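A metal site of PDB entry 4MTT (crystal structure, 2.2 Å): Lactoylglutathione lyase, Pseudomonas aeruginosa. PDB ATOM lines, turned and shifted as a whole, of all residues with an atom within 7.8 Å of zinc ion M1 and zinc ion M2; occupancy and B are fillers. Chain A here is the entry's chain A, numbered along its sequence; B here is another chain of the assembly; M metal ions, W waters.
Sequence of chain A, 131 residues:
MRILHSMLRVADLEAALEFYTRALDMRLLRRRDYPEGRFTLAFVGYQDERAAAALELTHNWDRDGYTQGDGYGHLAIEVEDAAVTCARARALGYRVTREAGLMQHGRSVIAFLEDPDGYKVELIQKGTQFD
The nearest printed residue that does not touch zinc ion M1 is Ala 76 of chain B (4.3 Å).
Zinc ion M2 is bound by water W1 (1.9 Å), the side-chain carboxylate of Glu 122 of chain B (2.0 Å), a ring nitrogen (NE2) of His 105 of chain B (2.0 Å) and water W2 (2.1 Å).
Zinc ion M2 has four donor atoms within binding distance.
N of Glu 122 of chain B lies within hydrogen-bond range of O of Leu 75 of chain B, at 2.8 Å.
O of Glu 122 of chain B lies within hydrogen-bond range of N of Ile 77 of chain B (2.8 Å).
The backbone NH (N) of Ala 76 of chain B is in hydrogen-bond range of the backbone carbonyl oxygen (O) of His 5 (2.8 Å).
The backbone NH (N) of Met 7 lies within hydrogen-bond range of the backbone carbonyl oxygen (O) of His 74 of chain B (2.7 Å).
O of Ser 6 lies within hydrogen-bond range of N of Glu 56, at 2.8 Å.
The backbone NH (N) of Leu 8 sits at hydrogen-bond distance from the backbone carbonyl oxygen (O) of Glu 56, 2.8 Å away.
Zinc ion M1 is bound by a ring nitrogen (NE2) of His 5 (2.0 Å), the side-chain carboxylate of Glu 122 of chain B (2.1 Å), water W1 (2.1 Å), a ring nitrogen (NE2) of His 74 of chain B (2.1 Å) and the side-chain carboxylate of Glu 56 (2.2 Å).
Zinc ion M1 has five donor atoms within binding distance.
Of the 23 residues printed, 2 come within 4 Å of zinc ion M2.
The nearest printed residue that does not touch zinc ion M2 is His 74 of chain B (4.3 Å).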
ATOM      1  N   LEU A   4     -18.227 -24.815  26.053  1.00  0.00           N
ATOM      2  CA  LEU A   4     -18.673 -25.413  24.781  1.00  0.00           C
ATOM      3  C   LEU A   4     -18.230 -24.659  23.545  1.00  0.00           C
ATOM      4  O   LEU A   4     -17.710 -25.263  22.618  1.00  0.00           O
ATOM      5  CB  LEU A   4     -20.209 -25.660  24.755  1.00  0.00           C
ATOM      6  CG  LEU A   4     -20.727 -26.706  25.736  1.00  0.00           C
ATOM      7  CD1 LEU A   4     -22.236 -26.657  25.852  1.00  0.00           C
ATOM      8  CD2 LEU A   4     -20.229 -28.115  25.393  1.00  0.00           C
ATOM      9  N   HIS A   5     -18.468 -23.352  23.511  1.00  0.00           N
ATOM     10  CA  HIS A   5     -18.127 -22.549  22.351  1.00  0.00           C
ATOM     11  C   HIS A   5     -18.208 -21.105  22.679  1.00  0.00           C
ATOM     12  O   HIS A   5     -18.795 -20.730  23.675  1.00  0.00           O
ATOM     13  CB  HIS A   5     -19.063 -22.856  21.122  1.00  0.00           C
ATOM     14  CG  HIS A   5     -20.530 -22.641  21.364  1.00  0.00           C
ATOM     15  ND1 HIS A   5     -21.372 -23.714  21.646  1.00  0.00           N
ATOM     16  CD2 HIS A   5     -21.257 -21.510  21.301  1.00  0.00           C
ATOM     17  CE1 HIS A   5     -22.588 -23.187  21.746  1.00  0.00           C
ATOM     18  NE2 HIS A   5     -22.564 -21.867  21.574  1.00  0.00           N
ATOM     19  N   SER A   6     -17.605 -20.286  21.816  1.00  0.00           N
ATOM     20  CA  SER A   6     -17.670 -18.834  21.809  1.00  0.00           C
ATOM     21  C   SER A   6     -18.449 -18.499  20.497  1.00  0.00           C
ATOM     22  O   SER A   6     -18.145 -19.059  19.452  1.00  0.00           O
ATOM     23  CB  SER A   6     -16.275 -18.243  21.734  1.00  0.00           C
ATOM     24  OG  SER A   6     -16.350 -16.831  21.729  1.00  0.00           O
ATOM     25  N   MET A   7     -19.469 -17.632  20.585  1.00  0.00           N
ATOM     26  CA  MET A   7     -20.247 -17.244  19.416  1.00  0.00           C
ATOM     27  C   MET A   7     -19.907 -15.837  18.932  1.00  0.00           C
ATOM     28  O   MET A   7     -19.889 -14.928  19.734  1.00  0.00           O
ATOM     29  CB  MET A   7     -21.760 -17.410  19.659  1.00  0.00           C
ATOM     30  CG  MET A   7     -22.616 -17.258  18.343  1.00  0.00           C
ATOM     31  SD  MET A   7     -22.951 -15.556  17.833  1.00  0.00           S
ATOM     32  CE  MET A   7     -24.483 -15.263  18.642  1.00  0.00           C
ATOM     33  N   LEU A   8     -19.652 -15.684  17.617  1.00  0.00           N
ATOM     34  CA  LEU A   8     -19.395 -14.415  16.925  1.00  0.00           C
ATOM     35  C   LEU A   8     -20.347 -14.253  15.735  1.00  0.00           C
ATOM     36  O   LEU A   8     -20.603 -15.211  14.998  1.00  0.00           O
ATOM     37  CB  LEU A   8     -17.940 -14.310  16.394  1.00  0.00           C
ATOM     38  CG  LEU A   8     -16.794 -14.374  17.443  1.00  0.00           C
ATOM     39  CD1 LEU A   8     -15.473 -14.293  16.760  1.00  0.00           C
ATOM     40  CD2 LEU A   8     -16.916 -13.262  18.517  1.00  0.00           C
ATOM     41  N   ARG A  30     -20.057 -28.540  12.053  1.00  0.00           N
ATOM     42  CA  ARG A  30     -21.520 -28.630  11.953  1.00  0.00           C
ATOM     43  C   ARG A  30     -22.042 -27.316  11.366  1.00  0.00           C
ATOM     44  O   ARG A  30     -21.520 -26.256  11.677  1.00  0.00           O
ATOM     45  CB  ARG A  30     -22.111 -28.842  13.386  1.00  0.00           C
ATOM     46  CG  ARG A  30     -23.632 -28.631  13.572  1.00  0.00           C
ATOM     47  CD  ARG A  30     -24.149 -29.263  14.868  1.00  0.00           C
ATOM     48  NE  ARG A  30     -23.588 -28.664  16.098  1.00  0.00           N
ATOM     49  CZ  ARG A  30     -24.271 -27.918  16.957  1.00  0.00           C
ATOM     50  NH1 ARG A  30     -25.546 -27.618  16.718  1.00  0.00           N
ATOM     51  NH2 ARG A  30     -23.683 -27.437  18.043  1.00  0.00           N
ATOM     52  N   LEU A  41     -25.850 -21.013  11.223  1.00  0.00           N
ATOM     53  CA  LEU A  41     -24.809 -21.196  12.238  1.00  0.00           C
ATOM     54  C   LEU A  41     -23.818 -22.171  11.660  1.00  0.00           C
ATOM     55  O   LEU A  41     -24.226 -23.164  11.046  1.00  0.00           O
ATOM     56  CB  LEU A  41     -25.306 -21.800  13.546  1.00  0.00           C
ATOM     57  CG  LEU A  41     -26.543 -21.259  14.147  1.00  0.00           C
ATOM     58  CD1 LEU A  41     -27.095 -22.257  15.102  1.00  0.00           C
ATOM     59  CD2 LEU A  41     -26.271 -19.875  14.810  1.00  0.00           C
ATOM     60  N   PHE A  43     -20.221 -24.144  13.157  1.00  0.00           N
ATOM     61  CA  PHE A  43     -19.284 -24.449  14.223  1.00  0.00           C
ATOM     62  C   PHE A  43     -17.996 -24.940  13.589  1.00  0.00           C
ATOM     63  O   PHE A  43     -18.012 -25.938  12.899  1.00  0.00           O
ATOM     64  CB  PHE A  43     -19.875 -25.510  15.181  1.00  0.00           C
ATOM     65  CG  PHE A  43     -21.036 -24.995  16.001  1.00  0.00           C
ATOM     66  CD1 PHE A  43     -22.328 -25.008  15.497  1.00  0.00           C
ATOM     67  CD2 PHE A  43     -20.834 -24.529  17.301  1.00  0.00           C
ATOM     68  CE1 PHE A  43     -23.401 -24.566  16.274  1.00  0.00           C
ATOM     69  CE2 PHE A  43     -21.913 -24.133  18.087  1.00  0.00           C
ATOM     70  CZ  PHE A  43     -23.186 -24.120  17.564  1.00  0.00           C
ATOM     71  N   GLU A  56     -18.432 -20.738  17.240  1.00  0.00           N
ATOM     72  CA  GLU A  56     -19.752 -20.640  16.630  1.00  0.00           C
ATOM     73  C   GLU A  56     -19.827 -19.337  15.827  1.00  0.00           C
ATOM     74  O   GLU A  56     -19.648 -18.256  16.398  1.00  0.00           O
ATOM     75  CB  GLU A  56     -20.865 -20.678  17.710  1.00  0.00           C
ATOM     76  CG  GLU A  56     -22.280 -20.619  17.142  1.00  0.00           C
ATOM     77  CD  GLU A  56     -23.453 -20.643  18.112  1.00  0.00           C
ATOM     78  OE1 GLU A  56     -23.260 -20.405  19.329  1.00  0.00           O
ATOM     79  OE2 GLU A  56     -24.591 -20.796  17.627  1.00  0.00           O
ATOM     80  N   THR A  58     -22.289 -17.027  13.515  1.00  0.00           N
ATOM     81  CA  THR A  58     -23.719 -16.777  13.272  1.00  0.00           C
ATOM     82  C   THR A  58     -23.871 -15.802  12.130  1.00  0.00           C
ATOM     83  O   THR A  58     -23.251 -14.717  12.126  1.00  0.00           O
ATOM     84  CB  THR A  58     -24.424 -16.258  14.533  1.00  0.00           C
ATOM     85  OG1 THR A  58     -24.357 -17.258  15.534  1.00  0.00           O
ATOM     86  CG2 THR A  58     -25.880 -15.905  14.291  1.00  0.00           C
ATOM     87  N   GLY B  73     -21.178 -12.487  20.419  1.00  0.00           N
ATOM     88  CA  GLY B  73     -22.363 -13.221  20.836  1.00  0.00           C
ATOM     89  C   GLY B  73     -22.444 -13.620  22.285  1.00  0.00           C
ATOM     90  O   GLY B  73     -23.144 -12.992  23.085  1.00  0.00           O
ATOM     91  N   HIS B  74     -21.788 -14.742  22.616  1.00  0.00           N
ATOM     92  CA  HIS B  74     -21.832 -15.335  23.953  1.00  0.00           C
ATOM     93  C   HIS B  74     -20.784 -16.440  24.083  1.00  0.00           C
ATOM     94  O   HIS B  74     -20.128 -16.817  23.116  1.00  0.00           O
ATOM     95  CB  HIS B  74     -23.254 -15.916  24.212  1.00  0.00           C
ATOM     96  CG  HIS B  74     -23.711 -16.930  23.192  1.00  0.00           C
ATOM     97  ND1 HIS B  74     -24.722 -16.631  22.269  1.00  0.00           N
ATOM     98  CD2 HIS B  74     -23.315 -18.212  23.004  1.00  0.00           C
ATOM     99  CE1 HIS B  74     -24.905 -17.735  21.566  1.00  0.00           C
ATOM    100  NE2 HIS B  74     -24.061 -18.713  21.957  1.00  0.00           N
ATOM    101  N   LEU B  75     -20.656 -16.961  25.315  1.00  0.00           N
ATOM    102  CA  LEU B  75     -19.838 -18.087  25.685  1.00  0.00           C
ATOM    103  C   LEU B  75     -20.840 -19.127  26.166  1.00  0.00           C
ATOM    104  O   LEU B  75     -21.681 -18.831  27.010  1.00  0.00           O
ATOM    105  CB  LEU B  75     -18.863 -17.715  26.859  1.00  0.00           C
ATOM    106  CG  LEU B  75     -17.843 -18.829  27.214  1.00  0.00           C
ATOM    107  CD1 LEU B  75     -16.818 -19.016  26.103  1.00  0.00           C
ATOM    108  CD2 LEU B  75     -17.106 -18.509  28.507  1.00  0.00           C
ATOM    109  N   ALA B  76     -20.792 -20.329  25.584  1.00  0.00           N
ATOM    110  CA  ALA B  76     -21.699 -21.397  26.011  1.00  0.00           C
ATOM    111  C   ALA B  76     -20.998 -22.340  26.968  1.00  0.00           C
ATOM    112  O   ALA B  76     -19.823 -22.677  26.778  1.00  0.00           O
ATOM    113  CB  ALA B  76     -22.223 -22.167  24.818  1.00  0.00           C
ATOM    114  N   ILE B  77     -21.735 -22.784  27.981  1.00  0.00           N
ATOM    115  CA  ILE B  77     -21.219 -23.687  29.000  1.00  0.00           C
ATOM    116  C   ILE B  77     -22.162 -24.866  29.184  1.00  0.00           C
ATOM    117  O   ILE B  77     -23.377 -24.705  29.196  1.00  0.00           O
ATOM    118  CB  ILE B  77     -20.972 -22.878  30.298  1.00  0.00           C
ATOM    119  CG1 ILE B  77     -19.597 -22.133  30.190  1.00  0.00           C
ATOM    120  CG2 ILE B  77     -21.023 -23.758  31.545  1.00  0.00           C
ATOM    121  CD1 ILE B  77     -19.555 -20.893  30.878  1.00  0.00           C
ATOM    122  N   LEU B 102     -35.813 -21.214  19.904  1.00  0.00           N
ATOM    123  CA  LEU B 102     -34.555 -21.021  19.165  1.00  0.00           C
ATOM    124  C   LEU B 102     -34.444 -22.279  18.324  1.00  0.00           C
ATOM    125  O   LEU B 102     -34.278 -23.371  18.885  1.00  0.00           O
ATOM    126  CB  LEU B 102     -33.317 -20.824  20.086  1.00  0.00           C
ATOM    127  CG  LEU B 102     -33.265 -19.521  20.921  1.00  0.00           C
ATOM    128  CD1 LEU B 102     -32.098 -19.543  21.964  1.00  0.00           C
ATOM    129  CD2 LEU B 102     -33.217 -18.241  20.023  1.00  0.00           C
ATOM    130  N   GLN B 104     -32.326 -23.513  16.540  1.00  0.00           N
ATOM    131  CA  GLN B 104     -31.036 -24.189  16.689  1.00  0.00           C
ATOM    132  C   GLN B 104     -30.996 -25.042  17.959  1.00  0.00           C
ATOM    133  O   GLN B 104     -30.090 -25.854  18.118  1.00  0.00           O
ATOM    134  CB  GLN B 104     -29.850 -23.207  16.621  1.00  0.00           C
ATOM    135  CG  GLN B 104     -29.750 -22.148  17.743  1.00  0.00           C
ATOM    136  CD  GLN B 104     -30.566 -20.906  17.452  1.00  0.00           C
ATOM    137  OE1 GLN B 104     -31.762 -20.964  17.126  1.00  0.00           O
ATOM    138  NE2 GLN B 104     -29.948 -19.748  17.597  1.00  0.00           N
ATOM    139  N   HIS B 105     -32.002 -24.907  18.843  1.00  0.00           N
ATOM    140  CA  HIS B 105     -32.031 -25.699  20.091  1.00  0.00           C
ATOM    141  C   HIS B 105     -33.286 -26.630  20.214  1.00  0.00           C
ATOM    142  O   HIS B 105     -33.618 -27.074  21.321  1.00  0.00           O
ATOM    143  CB  HIS B 105     -31.822 -24.809  21.321  1.00  0.00           C
ATOM    144  CG  HIS B 105     -30.487 -24.119  21.352  1.00  0.00           C
ATOM    145  ND1 HIS B 105     -29.322 -24.787  21.743  1.00  0.00           N
ATOM    146  CD2 HIS B 105     -30.162 -22.830  21.081  1.00  0.00           C
ATOM    147  CE1 HIS B 105     -28.341 -23.893  21.659  1.00  0.00           C
ATOM    148  NE2 HIS B 105     -28.803 -22.697  21.282  1.00  0.00           N
ATOM    149  N   ILE B 110     -33.728 -22.125  26.342  1.00  0.00           N
ATOM    150  CA  ILE B 110     -32.324 -21.874  26.728  1.00  0.00           C
ATOM    151  C   ILE B 110     -32.203 -20.659  27.620  1.00  0.00           C
ATOM    152  O   ILE B 110     -32.692 -19.586  27.288  1.00  0.00           O
ATOM    153  CB  ILE B 110     -31.403 -21.759  25.471  1.00  0.00           C
ATOM    154  CG1 ILE B 110     -31.521 -23.019  24.555  1.00  0.00           C
ATOM    155  CG2 ILE B 110     -29.921 -21.379  25.800  1.00  0.00           C
ATOM    156  CD1 ILE B 110     -30.966 -24.369  25.119  1.00  0.00           C
ATOM    157  N   PHE B 112     -29.817 -17.772  29.529  1.00  0.00           N
ATOM    158  CA  PHE B 112     -28.637 -16.947  29.321  1.00  0.00           C
ATOM    159  C   PHE B 112     -28.338 -16.154  30.601  1.00  0.00           C
ATOM    160  O   PHE B 112     -29.205 -15.448  31.123  1.00  0.00           O
ATOM    161  CB  PHE B 112     -28.818 -15.990  28.124  1.00  0.00           C
ATOM    162  CG  PHE B 112     -28.840 -16.680  26.770  1.00  0.00           C
ATOM    163  CD1 PHE B 112     -27.682 -16.760  25.997  1.00  0.00           C
ATOM    164  CD2 PHE B 112     -30.011 -17.219  26.259  1.00  0.00           C
ATOM    165  CE1 PHE B 112     -27.703 -17.386  24.739  1.00  0.00           C
ATOM    166  CE2 PHE B 112     -30.032 -17.837  25.008  1.00  0.00           C
ATOM    167  CZ  PHE B 112     -28.883 -17.925  24.262  1.00  0.00           C
ATOM    168  N   GLU B 122     -24.360 -18.592  27.695  1.00  0.00           N
ATOM    169  CA  GLU B 122     -25.367 -19.557  27.290  1.00  0.00           C
ATOM    170  C   GLU B 122     -25.265 -20.845  28.088  1.00  0.00           C
ATOM    171  O   GLU B 122     -24.208 -21.480  28.156  1.00  0.00           O
ATOM    172  CB  GLU B 122     -25.258 -19.800  25.779  1.00  0.00           C
ATOM    173  CG  GLU B 122     -26.137 -20.919  25.267  1.00  0.00           C
ATOM    174  CD  GLU B 122     -26.139 -20.980  23.761  1.00  0.00           C
ATOM    175  OE1 GLU B 122     -25.057 -21.218  23.162  1.00  0.00           O
ATOM    176  OE2 GLU B 122     -27.208 -20.737  23.173  1.00  0.00           O
ATOM    177  N   LEU B 123     -26.379 -21.246  28.723  1.00  0.00           N
ATOM    178  CA  LEU B 123     -26.387 -22.477  29.507  1.00  0.00           C
ATOM    179  C   LEU B 123     -26.964 -23.624  28.682  1.00  0.00           C
ATOM    180  O   LEU B 123     -28.093 -23.531  28.208  1.00  0.00           O
ATOM    181  CB  LEU B 123     -27.140 -22.321  30.828  1.00  0.00           C
ATOM    182  CG  LEU B 123     -26.689 -21.230  31.799  1.00  0.00           C
ATOM    183  CD1 LEU B 123     -27.508 -21.286  33.071  1.00  0.00           C
ATOM    184  CD2 LEU B 123     -25.161 -21.378  32.180  1.00  0.00           C
ATOM    185  N   ILE B 124     -26.179 -24.666  28.480  1.00  0.00           N
ATOM    186  CA  ILE B 124     -26.591 -25.856  27.761  1.00  0.00           C
ATOM    187  C   ILE B 124     -26.555 -27.020  28.747  1.00  0.00           C
ATOM    188  O   ILE B 124     -25.511 -27.336  29.333  1.00  0.00           O
ATOM    189  CB  ILE B 124     -25.795 -26.074  26.450  1.00  0.00           C
ATOM    190  CG1 ILE B 124     -26.129 -24.937  25.426  1.00  0.00           C
ATOM    191  CG2 ILE B 124     -26.117 -27.476  25.845  1.00  0.00           C
ATOM    192  CD1 ILE B 124     -25.108 -24.627  24.398  1.00  0.00           C
HETATM  193 ZN    ZN M   1     -24.178 -20.737  21.298  1.00  0.00          ZN
HETATM  194 ZN    ZN M   2     -27.491 -21.134  21.259  1.00  0.00          ZN
HETATM  195  O   HOH W   1     -25.907 -21.493  20.319  1.00  0.00           O
HETATM  196  O   HOH W   2     -28.455 -19.420  20.415  1.00  0.00           O
